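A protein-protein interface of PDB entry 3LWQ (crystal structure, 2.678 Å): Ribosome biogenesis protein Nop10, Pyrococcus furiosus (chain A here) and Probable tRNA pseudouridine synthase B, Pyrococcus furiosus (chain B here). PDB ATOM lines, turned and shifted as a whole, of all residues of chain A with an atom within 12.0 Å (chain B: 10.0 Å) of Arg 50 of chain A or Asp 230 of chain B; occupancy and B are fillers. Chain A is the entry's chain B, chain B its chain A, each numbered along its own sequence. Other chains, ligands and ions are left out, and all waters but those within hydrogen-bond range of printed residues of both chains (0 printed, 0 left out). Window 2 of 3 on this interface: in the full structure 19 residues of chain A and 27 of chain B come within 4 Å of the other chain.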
ATOM      1  N   ASP A  39      22.780   1.932   6.271  1.00  0.00           N
ATOM      2  CA  ASP A  39      22.785   1.005   5.143  1.00  0.00           C
ATOM      3  C   ASP A  39      21.579   1.225   4.237  1.00  0.00           C
ATOM      4  O   ASP A  39      20.626   0.443   4.251  1.00  0.00           O
ATOM      5  CB  ASP A  39      22.833  -0.440   5.640  1.00  0.00           C
ATOM      6  CG  ASP A  39      23.486  -1.376   4.645  1.00  0.00           C
ATOM      7  OD1 ASP A  39      24.250  -0.890   3.791  1.00  0.00           O
ATOM      8  OD2 ASP A  39      23.240  -2.597   4.721  1.00  0.00           O
ATOM      9  N   TYR A  41      21.225   1.060   1.009  1.00  0.00           N
ATOM     10  CA  TYR A  41      21.053   0.166  -0.124  1.00  0.00           C
ATOM     11  C   TYR A  41      21.271  -1.288   0.266  1.00  0.00           C
ATOM     12  O   TYR A  41      21.529  -2.134  -0.587  1.00  0.00           O
ATOM     13  CB  TYR A  41      22.004   0.545  -1.260  1.00  0.00           C
ATOM     14  CG  TYR A  41      22.178   2.029  -1.448  1.00  0.00           C
ATOM     15  CD1 TYR A  41      23.439   2.575  -1.674  1.00  0.00           C
ATOM     16  CD2 TYR A  41      21.089   2.891  -1.401  1.00  0.00           C
ATOM     17  CE1 TYR A  41      23.615   3.943  -1.852  1.00  0.00           C
ATOM     18  CE2 TYR A  41      21.249   4.262  -1.575  1.00  0.00           C
ATOM     19  CZ  TYR A  41      22.518   4.785  -1.801  1.00  0.00           C
ATOM     20  OH  TYR A  41      22.689   6.147  -1.975  1.00  0.00           O
ATOM     21  N   GLY A  42      21.179  -1.577   1.559  1.00  0.00           N
ATOM     22  CA  GLY A  42      21.272  -2.950   2.029  1.00  0.00           C
ATOM     23  C   GLY A  42      20.269  -3.812   1.283  1.00  0.00           C
ATOM     24  O   GLY A  42      20.604  -4.902   0.818  1.00  0.00           O
ATOM     25  N   GLU A  43      19.041  -3.302   1.148  1.00  0.00           N
ATOM     26  CA  GLU A  43      17.971  -3.997   0.433  1.00  0.00           C
ATOM     27  C   GLU A  43      18.489  -4.550  -0.887  1.00  0.00           C
ATOM     28  O   GLU A  43      18.200  -5.688  -1.248  1.00  0.00           O
ATOM     29  CB  GLU A  43      16.765  -3.071   0.197  1.00  0.00           C
ATOM     30  CG  GLU A  43      15.477  -3.787  -0.293  1.00  0.00           C
ATOM     31  CD  GLU A  43      14.269  -2.845  -0.523  1.00  0.00           C
ATOM     32  OE1 GLU A  43      14.305  -1.676  -0.077  1.00  0.00           O
ATOM     33  OE2 GLU A  43      13.276  -3.284  -1.153  1.00  0.00           O
ATOM     34  N   TYR A  44      19.296  -3.759  -1.583  1.00  0.00           N
ATOM     35  CA  TYR A  44      19.658  -4.080  -2.962  1.00  0.00           C
ATOM     36  C   TYR A  44      20.961  -4.853  -3.086  1.00  0.00           C
ATOM     37  O   TYR A  44      21.108  -5.710  -3.954  1.00  0.00           O
ATOM     38  CB  TYR A  44      19.632  -2.815  -3.842  1.00  0.00           C
ATOM     39  CG  TYR A  44      18.215  -2.296  -3.983  1.00  0.00           C
ATOM     40  CD1 TYR A  44      17.669  -1.445  -3.028  1.00  0.00           C
ATOM     41  CD2 TYR A  44      17.403  -2.704  -5.039  1.00  0.00           C
ATOM     42  CE1 TYR A  44      16.360  -0.990  -3.132  1.00  0.00           C
ATOM     43  CE2 TYR A  44      16.094  -2.252  -5.154  1.00  0.00           C
ATOM     44  CZ  TYR A  44      15.576  -1.394  -4.195  1.00  0.00           C
ATOM     45  OH  TYR A  44      14.274  -0.937  -4.299  1.00  0.00           O
ATOM     46  N   ARG A  45      21.904  -4.552  -2.210  1.00  0.00           N
ATOM     47  CA  ARG A  45      23.120  -5.332  -2.140  1.00  0.00           C
ATOM     48  C   ARG A  45      22.743  -6.797  -1.937  1.00  0.00           C
ATOM     49  O   ARG A  45      23.111  -7.667  -2.730  1.00  0.00           O
ATOM     50  CB  ARG A  45      23.948  -4.843  -0.962  1.00  0.00           C
ATOM     51  CG  ARG A  45      25.352  -5.378  -0.908  1.00  0.00           C
ATOM     52  CD  ARG A  45      26.076  -4.722   0.231  1.00  0.00           C
ATOM     53  NE  ARG A  45      25.535  -5.073   1.544  1.00  0.00           N
ATOM     54  CZ  ARG A  45      24.970  -4.206   2.382  1.00  0.00           C
ATOM     55  NH1 ARG A  45      24.841  -2.926   2.042  1.00  0.00           N
ATOM     56  NH2 ARG A  45      24.532  -4.616   3.568  1.00  0.00           N
ATOM     57  N   ARG A  46      21.986  -7.049  -0.873  1.00  0.00           N
ATOM     58  CA  ARG A  46      21.462  -8.380  -0.579  1.00  0.00           C
ATOM     59  C   ARG A  46      20.870  -9.097  -1.785  1.00  0.00           C
ATOM     60  O   ARG A  46      21.124 -10.289  -1.974  1.00  0.00           O
ATOM     61  CB  ARG A  46      20.459  -8.345   0.581  1.00  0.00           C
ATOM     62  CG  ARG A  46      21.112  -8.377   1.982  1.00  0.00           C
ATOM     63  CD  ARG A  46      20.159  -7.879   3.061  1.00  0.00           C
ATOM     64  NE  ARG A  46      20.818  -6.886   3.900  1.00  0.00           N
ATOM     65  CZ  ARG A  46      20.226  -5.792   4.371  1.00  0.00           C
ATOM     66  NH1 ARG A  46      18.954  -5.541   4.076  1.00  0.00           N
ATOM     67  NH2 ARG A  46      20.912  -4.937   5.127  1.00  0.00           N
ATOM     68  N   ARG A  47      20.095  -8.396  -2.607  1.00  0.00           N
ATOM     69  CA  ARG A  47      19.582  -9.037  -3.823  1.00  0.00           C
ATOM     70  C   ARG A  47      20.707  -9.522  -4.733  1.00  0.00           C
ATOM     71  O   ARG A  47      20.734 -10.682  -5.167  1.00  0.00           O
ATOM     72  CB  ARG A  47      18.581  -8.152  -4.579  1.00  0.00           C
ATOM     73  CG  ARG A  47      17.168  -8.251  -3.990  1.00  0.00           C
ATOM     74  CD  ARG A  47      16.140  -7.401  -4.722  1.00  0.00           C
ATOM     75  NE  ARG A  47      15.100  -6.954  -3.798  1.00  0.00           N
ATOM     76  CZ  ARG A  47      14.201  -6.017  -4.080  1.00  0.00           C
ATOM     77  NH1 ARG A  47      14.201  -5.432  -5.275  1.00  0.00           N
ATOM     78  NH2 ARG A  47      13.301  -5.663  -3.166  1.00  0.00           N
ATOM     79  N   TRP A  48      21.652  -8.634  -4.998  1.00  0.00           N
ATOM     80  CA  TRP A  48      22.797  -9.003  -5.796  1.00  0.00           C
ATOM     81  C   TRP A  48      23.572 -10.138  -5.134  1.00  0.00           C
ATOM     82  O   TRP A  48      24.113 -11.013  -5.811  1.00  0.00           O
ATOM     83  CB  TRP A  48      23.688  -7.796  -5.991  1.00  0.00           C
ATOM     84  CG  TRP A  48      25.110  -8.150  -6.117  1.00  0.00           C
ATOM     85  CD1 TRP A  48      25.720  -8.756  -7.181  1.00  0.00           C
ATOM     86  CD2 TRP A  48      26.126  -7.926  -5.140  1.00  0.00           C
ATOM     87  NE1 TRP A  48      27.059  -8.923  -6.925  1.00  0.00           N
ATOM     88  CE2 TRP A  48      27.338  -8.417  -5.680  1.00  0.00           C
ATOM     89  CE3 TRP A  48      26.133  -7.348  -3.864  1.00  0.00           C
ATOM     90  CZ2 TRP A  48      28.546  -8.353  -4.987  1.00  0.00           C
ATOM     91  CZ3 TRP A  48      27.327  -7.295  -3.174  1.00  0.00           C
ATOM     92  CH2 TRP A  48      28.522  -7.791  -3.741  1.00  0.00           C
ATOM     93  N   LYS A  49      23.601 -10.131  -3.807  1.00  0.00           N
ATOM     94  CA  LYS A  49      24.411 -11.085  -3.051  1.00  0.00           C
ATOM     95  C   LYS A  49      23.826 -12.497  -3.032  1.00  0.00           C
ATOM     96  O   LYS A  49      24.558 -13.477  -3.176  1.00  0.00           O
ATOM     97  CB  LYS A  49      24.605 -10.582  -1.627  1.00  0.00           C
ATOM     98  CG  LYS A  49      25.528 -11.423  -0.782  1.00  0.00           C
ATOM     99  CD  LYS A  49      25.965 -10.655   0.465  1.00  0.00           C
ATOM    100  CE  LYS A  49      27.160  -9.741   0.168  1.00  0.00           C
ATOM    101  NZ  LYS A  49      27.656  -9.012   1.380  1.00  0.00           N
ATOM    102  N   ARG A  50      22.509 -12.582  -2.838  1.00  0.00           N
ATOM    103  CA  ARG A  50      21.774 -13.844  -2.843  1.00  0.00           C
ATOM    104  C   ARG A  50      21.925 -14.605  -4.151  1.00  0.00           C
ATOM    105  O   ARG A  50      21.825 -15.829  -4.171  1.00  0.00           O
ATOM    106  CB  ARG A  50      20.286 -13.591  -2.621  1.00  0.00           C
ATOM    107  CG  ARG A  50      19.894 -13.359  -1.190  1.00  0.00           C
ATOM    108  CD  ARG A  50      18.402 -13.209  -1.063  1.00  0.00           C
ATOM    109  NE  ARG A  50      18.018 -12.680   0.242  1.00  0.00           N
ATOM    110  CZ  ARG A  50      17.615 -11.430   0.448  1.00  0.00           C
ATOM    111  NH1 ARG A  50      17.549 -10.583  -0.578  1.00  0.00           N
ATOM    112  NH2 ARG A  50      17.275 -11.028   1.674  1.00  0.00           N
ATOM    113  N   GLU A  51      22.137 -13.880  -5.245  1.00  0.00           N
ATOM    114  CA  GLU A  51      22.237 -14.511  -6.546  1.00  0.00           C
ATOM    115  C   GLU A  51      23.591 -15.181  -6.668  1.00  0.00           C
ATOM    116  O   GLU A  51      23.707 -16.283  -7.203  1.00  0.00           O
ATOM    117  CB  GLU A  51      22.029 -13.498  -7.676  1.00  0.00           C
ATOM    118  CG  GLU A  51      21.742 -14.153  -9.026  1.00  0.00           C
ATOM    119  CD  GLU A  51      21.085 -13.207 -10.022  1.00  0.00           C
ATOM    120  OE1 GLU A  51      21.169 -11.976  -9.816  1.00  0.00           O
ATOM    121  OE2 GLU A  51      20.487 -13.695 -11.008  1.00  0.00           O
ATOM    122  N   VAL A  52      24.615 -14.515  -6.157  1.00  0.00           N
ATOM    123  CA  VAL A  52      25.963 -15.067  -6.183  1.00  0.00           C
ATOM    124  C   VAL A  52      26.066 -16.300  -5.271  1.00  0.00           C
ATOM    125  O   VAL A  52      27.100 -16.968  -5.233  1.00  0.00           O
ATOM    126  CB  VAL A  52      27.015 -14.012  -5.732  1.00  0.00           C
ATOM    127  CG1 VAL A  52      28.367 -14.309  -6.347  1.00  0.00           C
ATOM    128  CG2 VAL A  52      26.580 -12.614  -6.114  1.00  0.00           C
ATOM    129  N   LEU A  53      24.990 -16.608  -4.549  1.00  0.00           N
ATOM    130  CA  LEU A  53      25.034 -17.671  -3.548  1.00  0.00           C
ATOM    131  C   LEU A  53      23.935 -18.744  -3.667  1.00  0.00           C
ATOM    132  O   LEU A  53      24.207 -19.933  -3.491  1.00  0.00           O
ATOM    133  CB  LEU A  53      25.026 -17.069  -2.142  1.00  0.00           C
ATOM    134  CG  LEU A  53      26.065 -15.994  -1.816  1.00  0.00           C
ATOM    135  CD1 LEU A  53      25.974 -15.607  -0.347  1.00  0.00           C
ATOM    136  CD2 LEU A  53      27.464 -16.462  -2.146  1.00  0.00           C
ATOM    137  N   GLY A  54      22.699 -18.324  -3.931  1.00  0.00           N
ATOM    138  CA  GLY A  54      21.586 -19.249  -4.076  1.00  0.00           C
ATOM    139  C   GLY A  54      20.565 -19.184  -2.954  1.00  0.00           C
ATOM    140  O   GLY A  54      20.458 -18.187  -2.236  1.00  0.00           O
ATOM    141  N   ASP B 219      29.181  -8.331   4.968  1.00  0.00           N
ATOM    142  CA  ASP B 219      28.919  -9.774   5.049  1.00  0.00           C
ATOM    143  C   ASP B 219      28.162 -10.114   6.326  1.00  0.00           C
ATOM    144  O   ASP B 219      27.110 -10.755   6.291  1.00  0.00           O
ATOM    145  CB  ASP B 219      30.208 -10.591   4.987  1.00  0.00           C
ATOM    146  CG  ASP B 219      30.867 -10.549   3.612  1.00  0.00           C
ATOM    147  OD1 ASP B 219      30.143 -10.354   2.610  1.00  0.00           O
ATOM    148  OD2 ASP B 219      32.110 -10.714   3.539  1.00  0.00           O
ATOM    149  N   VAL B 221      26.265  -8.247   8.516  1.00  0.00           N
ATOM    150  CA  VAL B 221      24.848  -7.848   8.580  1.00  0.00           C
ATOM    151  C   VAL B 221      24.005  -8.536   7.513  1.00  0.00           C
ATOM    152  O   VAL B 221      22.822  -8.807   7.732  1.00  0.00           O
ATOM    153  CB  VAL B 221      24.577  -6.313   8.503  1.00  0.00           C
ATOM    154  CG1 VAL B 221      25.249  -5.580   9.655  1.00  0.00           C
ATOM    155  CG2 VAL B 221      24.974  -5.758   7.170  1.00  0.00           C
ATOM    156  N   ASP B 222      24.605  -8.825   6.364  1.00  0.00           N
ATOM    157  CA  ASP B 222      23.872  -9.564   5.339  1.00  0.00           C
ATOM    158  C   ASP B 222      23.615 -11.000   5.769  1.00  0.00           C
ATOM    159  O   ASP B 222      22.488 -11.460   5.729  1.00  0.00           O
ATOM    160  CB  ASP B 222      24.597  -9.521   4.007  1.00  0.00           C
ATOM    161  CG  ASP B 222      24.517  -8.155   3.359  1.00  0.00           C
ATOM    162  OD1 ASP B 222      23.689  -7.336   3.830  1.00  0.00           O
ATOM    163  OD2 ASP B 222      25.277  -7.906   2.391  1.00  0.00           O
ATOM    164  N   TYR B 223      24.664 -11.687   6.208  1.00  0.00           N
ATOM    165  CA  TYR B 223      24.535 -13.038   6.751  1.00  0.00           C
ATOM    166  C   TYR B 223      23.466 -13.095   7.809  1.00  0.00           C
ATOM    167  O   TYR B 223      22.725 -14.067   7.904  1.00  0.00           O
ATOM    168  CB  TYR B 223      25.873 -13.495   7.323  1.00  0.00           C
ATOM    169  CG  TYR B 223      26.868 -13.738   6.226  1.00  0.00           C
ATOM    170  CD1 TYR B 223      26.534 -13.436   4.908  1.00  0.00           C
ATOM    171  CD2 TYR B 223      28.146 -14.231   6.491  1.00  0.00           C
ATOM    172  CE1 TYR B 223      27.413 -13.641   3.887  1.00  0.00           C
ATOM    173  CE2 TYR B 223      29.052 -14.451   5.453  1.00  0.00           C
ATOM    174  CZ  TYR B 223      28.670 -14.151   4.152  1.00  0.00           C
ATOM    175  OH  TYR B 223      29.525 -14.337   3.091  1.00  0.00           O
ATOM    176  N   TYR B 224      23.387 -12.033   8.599  1.00  0.00           N
ATOM    177  CA  TYR B 224      22.394 -11.933   9.657  1.00  0.00           C
ATOM    178  C   TYR B 224      20.996 -11.950   9.070  1.00  0.00           C
ATOM    179  O   TYR B 224      20.128 -12.659   9.561  1.00  0.00           O
ATOM    180  CB  TYR B 224      22.614 -10.652  10.464  1.00  0.00           C
ATOM    181  CG  TYR B 224      21.583 -10.418  11.557  1.00  0.00           C
ATOM    182  CD1 TYR B 224      21.633 -11.129  12.756  1.00  0.00           C
ATOM    183  CD2 TYR B 224      20.564  -9.480  11.395  1.00  0.00           C
ATOM    184  CE1 TYR B 224      20.695 -10.916  13.759  1.00  0.00           C
ATOM    185  CE2 TYR B 224      19.627  -9.258  12.397  1.00  0.00           C
ATOM    186  CZ  TYR B 224      19.691  -9.979  13.574  1.00  0.00           C
ATOM    187  OH  TYR B 224      18.749  -9.761  14.563  1.00  0.00           O
ATOM    188  N   TYR B 225      20.782 -11.182   8.005  1.00  0.00           N
ATOM    189  CA  TYR B 225      19.452 -11.053   7.417  1.00  0.00           C
ATOM    190  C   TYR B 225      19.081 -12.259   6.587  1.00  0.00           C
ATOM    191  O   TYR B 225      17.912 -12.618   6.503  1.00  0.00           O
ATOM    192  CB  TYR B 225      19.332  -9.787   6.572  1.00  0.00           C
ATOM    193  CG  TYR B 225      19.239  -8.525   7.387  1.00  0.00           C
ATOM    194  CD1 TYR B 225      20.241  -7.572   7.333  1.00  0.00           C
ATOM    195  CD2 TYR B 225      18.158  -8.294   8.226  1.00  0.00           C
ATOM    196  CE1 TYR B 225      20.167  -6.413   8.074  1.00  0.00           C
ATOM    197  CE2 TYR B 225      18.077  -7.138   8.976  1.00  0.00           C
ATOM    198  CZ  TYR B 225      19.087  -6.201   8.892  1.00  0.00           C
ATOM    199  OH  TYR B 225      19.022  -5.045   9.628  1.00  0.00           O
ATOM    200  N   PHE B 226      20.062 -12.896   5.966  1.00  0.00           N
ATOM    201  CA  PHE B 226      19.786 -14.185   5.350  1.00  0.00           C
ATOM    202  C   PHE B 226      19.295 -15.142   6.419  1.00  0.00           C
ATOM    203  O   PHE B 226      18.394 -15.939   6.182  1.00  0.00           O
ATOM    204  CB  PHE B 226      21.022 -14.772   4.688  1.00  0.00           C
ATOM    205  CG  PHE B 226      21.590 -13.908   3.626  1.00  0.00           C
ATOM    206  CD1 PHE B 226      22.883 -14.094   3.188  1.00  0.00           C
ATOM    207  CD2 PHE B 226      20.833 -12.886   3.078  1.00  0.00           C
ATOM    208  CE1 PHE B 226      23.404 -13.294   2.210  1.00  0.00           C
ATOM    209  CE2 PHE B 226      21.351 -12.081   2.106  1.00  0.00           C
ATOM    210  CZ  PHE B 226      22.633 -12.281   1.663  1.00  0.00           C
ATOM    211  N   TRP B 227      19.890 -15.074   7.601  1.00  0.00           N
ATOM    212  CA  TRP B 227      19.453 -15.982   8.636  1.00  0.00           C
ATOM    213  C   TRP B 227      18.089 -15.570   9.169  1.00  0.00           C
ATOM    214  O   TRP B 227      17.152 -16.354   9.138  1.00  0.00           O
ATOM    215  CB  TRP B 227      20.471 -16.105   9.763  1.00  0.00           C
ATOM    216  CG  TRP B 227      19.857 -16.706  10.949  1.00  0.00           C
ATOM    217  CD1 TRP B 227      19.068 -17.824  10.983  1.00  0.00           C
ATOM    218  CD2 TRP B 227      19.940 -16.226  12.292  1.00  0.00           C
ATOM    219  NE1 TRP B 227      18.665 -18.068  12.272  1.00  0.00           N
ATOM    220  CE2 TRP B 227      19.184 -17.102  13.094  1.00  0.00           C
ATOM    221  CE3 TRP B 227      20.586 -15.147  12.899  1.00  0.00           C
ATOM    222  CZ2 TRP B 227      19.058 -16.933  14.470  1.00  0.00           C
ATOM    223  CZ3 TRP B 227      20.456 -14.978  14.272  1.00  0.00           C
ATOM    224  CH2 TRP B 227      19.699 -15.867  15.040  1.00  0.00           C
ATOM    225  N   LYS B 228      17.975 -14.329   9.627  1.00  0.00           N
ATOM    226  CA  LYS B 228      16.733 -13.837  10.234  1.00  0.00           C
ATOM    227  C   LYS B 228      15.538 -13.726   9.282  1.00  0.00           C
ATOM    228  O   LYS B 228      14.420 -14.060   9.658  1.00  0.00           O
ATOM    229  CB  LYS B 228      16.964 -12.495  10.938  1.00  0.00           C
ATOM    230  CG  LYS B 228      17.319 -12.623  12.425  1.00  0.00           C
ATOM    231  CD  LYS B 228      16.052 -12.789  13.232  1.00  0.00           C
ATOM    232  CE  LYS B 228      16.298 -13.026  14.704  1.00  0.00           C
ATOM    233  NZ  LYS B 228      14.983 -12.923  15.403  1.00  0.00           N
ATOM    234  N   GLU B 229      15.763 -13.247   8.061  1.00  0.00           N
ATOM    235  CA  GLU B 229      14.651 -12.968   7.147  1.00  0.00           C
ATOM    236  C   GLU B 229      14.445 -14.033   6.058  1.00  0.00           C
ATOM    237  O   GLU B 229      13.347 -14.168   5.523  1.00  0.00           O
ATOM    238  CB  GLU B 229      14.787 -11.559   6.537  1.00  0.00           C
ATOM    239  CG  GLU B 229      14.422 -10.416   7.512  1.00  0.00           C
ATOM    240  CD  GLU B 229      14.565  -9.014   6.905  1.00  0.00           C
ATOM    241  OE1 GLU B 229      14.353  -8.020   7.640  1.00  0.00           O
ATOM    242  OE2 GLU B 229      14.893  -8.905   5.703  1.00  0.00           O
ATOM    243  N   ASP B 230      15.496 -14.794   5.758  1.00  0.00           N
ATOM    244  CA  ASP B 230      15.452 -15.824   4.724  1.00  0.00           C
ATOM    245  C   ASP B 230      15.296 -17.227   5.307  1.00  0.00           C
ATOM    246  O   ASP B 230      14.756 -18.108   4.643  1.00  0.00           O
ATOM    247  CB  ASP B 230      16.708 -15.788   3.841  1.00  0.00           C
ATOM    248  CG  ASP B 230      16.852 -14.491   3.063  1.00  0.00           C
ATOM    249  OD1 ASP B 230      16.955 -14.564   1.820  1.00  0.00           O
ATOM    250  OD2 ASP B 230      16.874 -13.405   3.686  1.00  0.00           O
ATOM    251  N   GLY B 231      15.773 -17.438   6.536  1.00  0.00           N
ATOM    252  CA  GLY B 231      15.629 -18.724   7.213  1.00  0.00           C
ATOM    253  C   GLY B 231      16.858 -19.616   7.105  1.00  0.00           C
ATOM    254  O   GLY B 231      16.870 -20.736   7.611  1.00  0.00           O
ATOM    255  N   ILE B 232      17.895 -19.095   6.455  1.00  0.00           N
ATOM    256  CA  ILE B 232      19.170 -19.780   6.251  1.00  0.00           C
ATOM    257  C   ILE B 232      20.230 -19.401   7.292  1.00  0.00           C
ATOM    258  O   ILE B 232      20.905 -18.366   7.164  1.00  0.00           O
ATOM    259  CB  ILE B 232      19.719 -19.404   4.883  1.00  0.00           C
ATOM    260  CG1 ILE B 232      18.730 -19.829   3.802  1.00  0.00           C
ATOM    261  CG2 ILE B 232      21.077 -20.030   4.669  1.00  0.00           C
ATOM    262  CD1 ILE B 232      18.776 -18.975   2.527  1.00  0.00           C
ATOM    263  N   GLU B 233      20.397 -20.234   8.315  1.00  0.00           N
ATOM    264  CA  GLU B 233      21.269 -19.865   9.434  1.00  0.00           C
ATOM    265  C   GLU B 233      22.748 -20.124   9.145  1.00  0.00           C
ATOM    266  O   GLU B 233      23.615 -19.775   9.945  1.00  0.00           O
ATOM    267  CB  GLU B 233      20.842 -20.578  10.725  1.00  0.00           C
ATOM    268  CG  GLU B 233      21.304 -22.027  10.837  1.00  0.00           C
ATOM    269  CD  GLU B 233      20.758 -22.729  12.075  1.00  0.00           C
ATOM    270  OE1 GLU B 233      21.566 -23.320  12.831  1.00  0.00           O
ATOM    271  OE2 GLU B 233      19.522 -22.686  12.289  1.00  0.00           O
ATOM    272  N   GLU B 234      23.017 -20.715   7.987  1.00  0.00           N
ATOM    273  CA  GLU B 234      24.335 -21.244   7.641  1.00  0.00           C
ATOM    274  C   GLU B 234      25.456 -20.209   7.604  1.00  0.00           C
ATOM    275  O   GLU B 234      26.446 -20.348   8.318  1.00  0.00           O
ATOM    276  CB  GLU B 234      24.258 -21.965   6.292  1.00  0.00           C
ATOM    277  CG  GLU B 234      25.600 -22.360   5.701  1.00  0.00           C
ATOM    278  CD  GLU B 234      25.477 -22.890   4.276  1.00  0.00           C
ATOM    279  OE1 GLU B 234      26.499 -22.876   3.550  1.00  0.00           O
ATOM    280  OE2 GLU B 234      24.359 -23.315   3.883  1.00  0.00           O
ATOM    281  N   TYR B 235      25.314 -19.190   6.760  1.00  0.00           N
ATOM    282  CA  TYR B 235      26.370 -18.201   6.593  1.00  0.00           C
ATOM    283  C   TYR B 235      26.590 -17.390   7.873  1.00  0.00           C
ATOM    284  O   TYR B 235      27.727 -17.037   8.204  1.00  0.00           O
ATOM    285  CB  TYR B 235      26.083 -17.299   5.396  1.00  0.00           C
ATOM    286  CG  TYR B 235      25.852 -18.089   4.130  1.00  0.00           C
ATOM    287  CD1 TYR B 235      24.578 -18.535   3.784  1.00  0.00           C
ATOM    288  CD2 TYR B 235      26.913 -18.420   3.292  1.00  0.00           C
ATOM    289  CE1 TYR B 235      24.364 -19.274   2.632  1.00  0.00           C
ATOM    290  CE2 TYR B 235      26.711 -19.161   2.136  1.00  0.00           C
ATOM    291  CZ  TYR B 235      25.436 -19.588   1.807  1.00  0.00           C
ATOM    292  OH  TYR B 235      25.243 -20.326   0.655  1.00  0.00           O
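Among the printed residues, pairs that only touch across the chains: Arg 45 of chain A with Val 221 of chain B (3.8 Å), Arg 46 of chain A with Tyr 225 of chain B (3.4 Å), Arg 46 of chain A with Phe 226 of chain B (3.7 Å), Lys 49 of chain A with Phe 226 of chain B (3.9 Å) and Arg 50 of chain A with Phe 226 of chain B (3.8 Å).
OD1 of Asp 219 of chain B lies within salt-bridge range of NZ of Lys 49 of chain A (3.1 Å).
NH2 of Arg 45 of chain A is in salt-bridge range of OD1 of Asp 222 of chain B, 2.9 Å away.
The side-chain carboxylate (OD1) of Asp 222 of chain B is in salt-bridge range of the guanidinium group (NE) of Arg 46 of chain A (2.9 Å).
The side-chain carboxylate (OD2) of Asp 222 of chain B is in salt-bridge range of the side-chain amino group (NZ) of Lys 49 of chain A (2.8 Å).
OD1 of Asp 230 of chain B is in salt-bridge range of NE of Arg 50 of chain A, 2.7 Å away.
The backbone carbonyl oxygen of Tyr 225 of chain B sits at hydrogen-bond distance from the backbone NH of Asp 230 of chain B (3.3 Å).
N of Gly 231 of chain B is in hydrogen-bond range of O of Phe 226 of chain B, 3.0 Å away.
The backbone NH (N) of Ile 232 of chain B lies within hydrogen-bond range of the backbone carbonyl oxygen (O) of Phe 226 of chain B.
NH2 of Arg 45 of chain A lies within salt-bridge range of OD2 of Asp 39 of chain A, at 2.7 Å.
OD2 of Asp 39 of chain A is in salt-bridge range of NH2 of Arg 46 of chain A (3.3 Å).
Tyr 44 of chain A touches none of the printed residues of chain B.
Printed residues of chain B within 4 Å of Lys 49 of chain A: Asp 219 (3.1 Å), Asp 222 (2.8 Å) and Phe 226 (3.9 Å).
Of chain B, only Phe 226 (3.8 Å) and Asp 230 (2.7 Å) come within 4 Å of Arg 50 of chain A.
No residue of chain B comes within 4 Å of Gly 54 of chain A.
Of the printed residues of chain A, Asp 219 of chain B touches Lys 49.
Printed residues of chain A within 4 Å of Val 221 of chain B: Arg 45.
Printed residues of chain A within 4 Å of Tyr 225 of chain B: Arg 46.
Of the printed residues of chain A, Phe 226 of chain B touches Arg 46, Lys 49 and Arg 50.
No residue of chain A comes within 4 Å of Glu 229 of chain B.
Asp 230 of chain B touches just one residue of chain A: Arg 50.
No residue of chain A comes within 4 Å of Gly 231 of chain B.
No residue of chain A comes within 4 Å of Ile 232 of chain B.
The nearest printed residue of chain A that does not touch Asp 230 of chain B is Arg 46 of chain A (6.5 Å).
Printed residues of chain A that touch a printed residue of chain B: Arg 45, Arg 46, Lys 49 and Arg 50.
Among the printed residues, 10 pairs touch across the chains.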
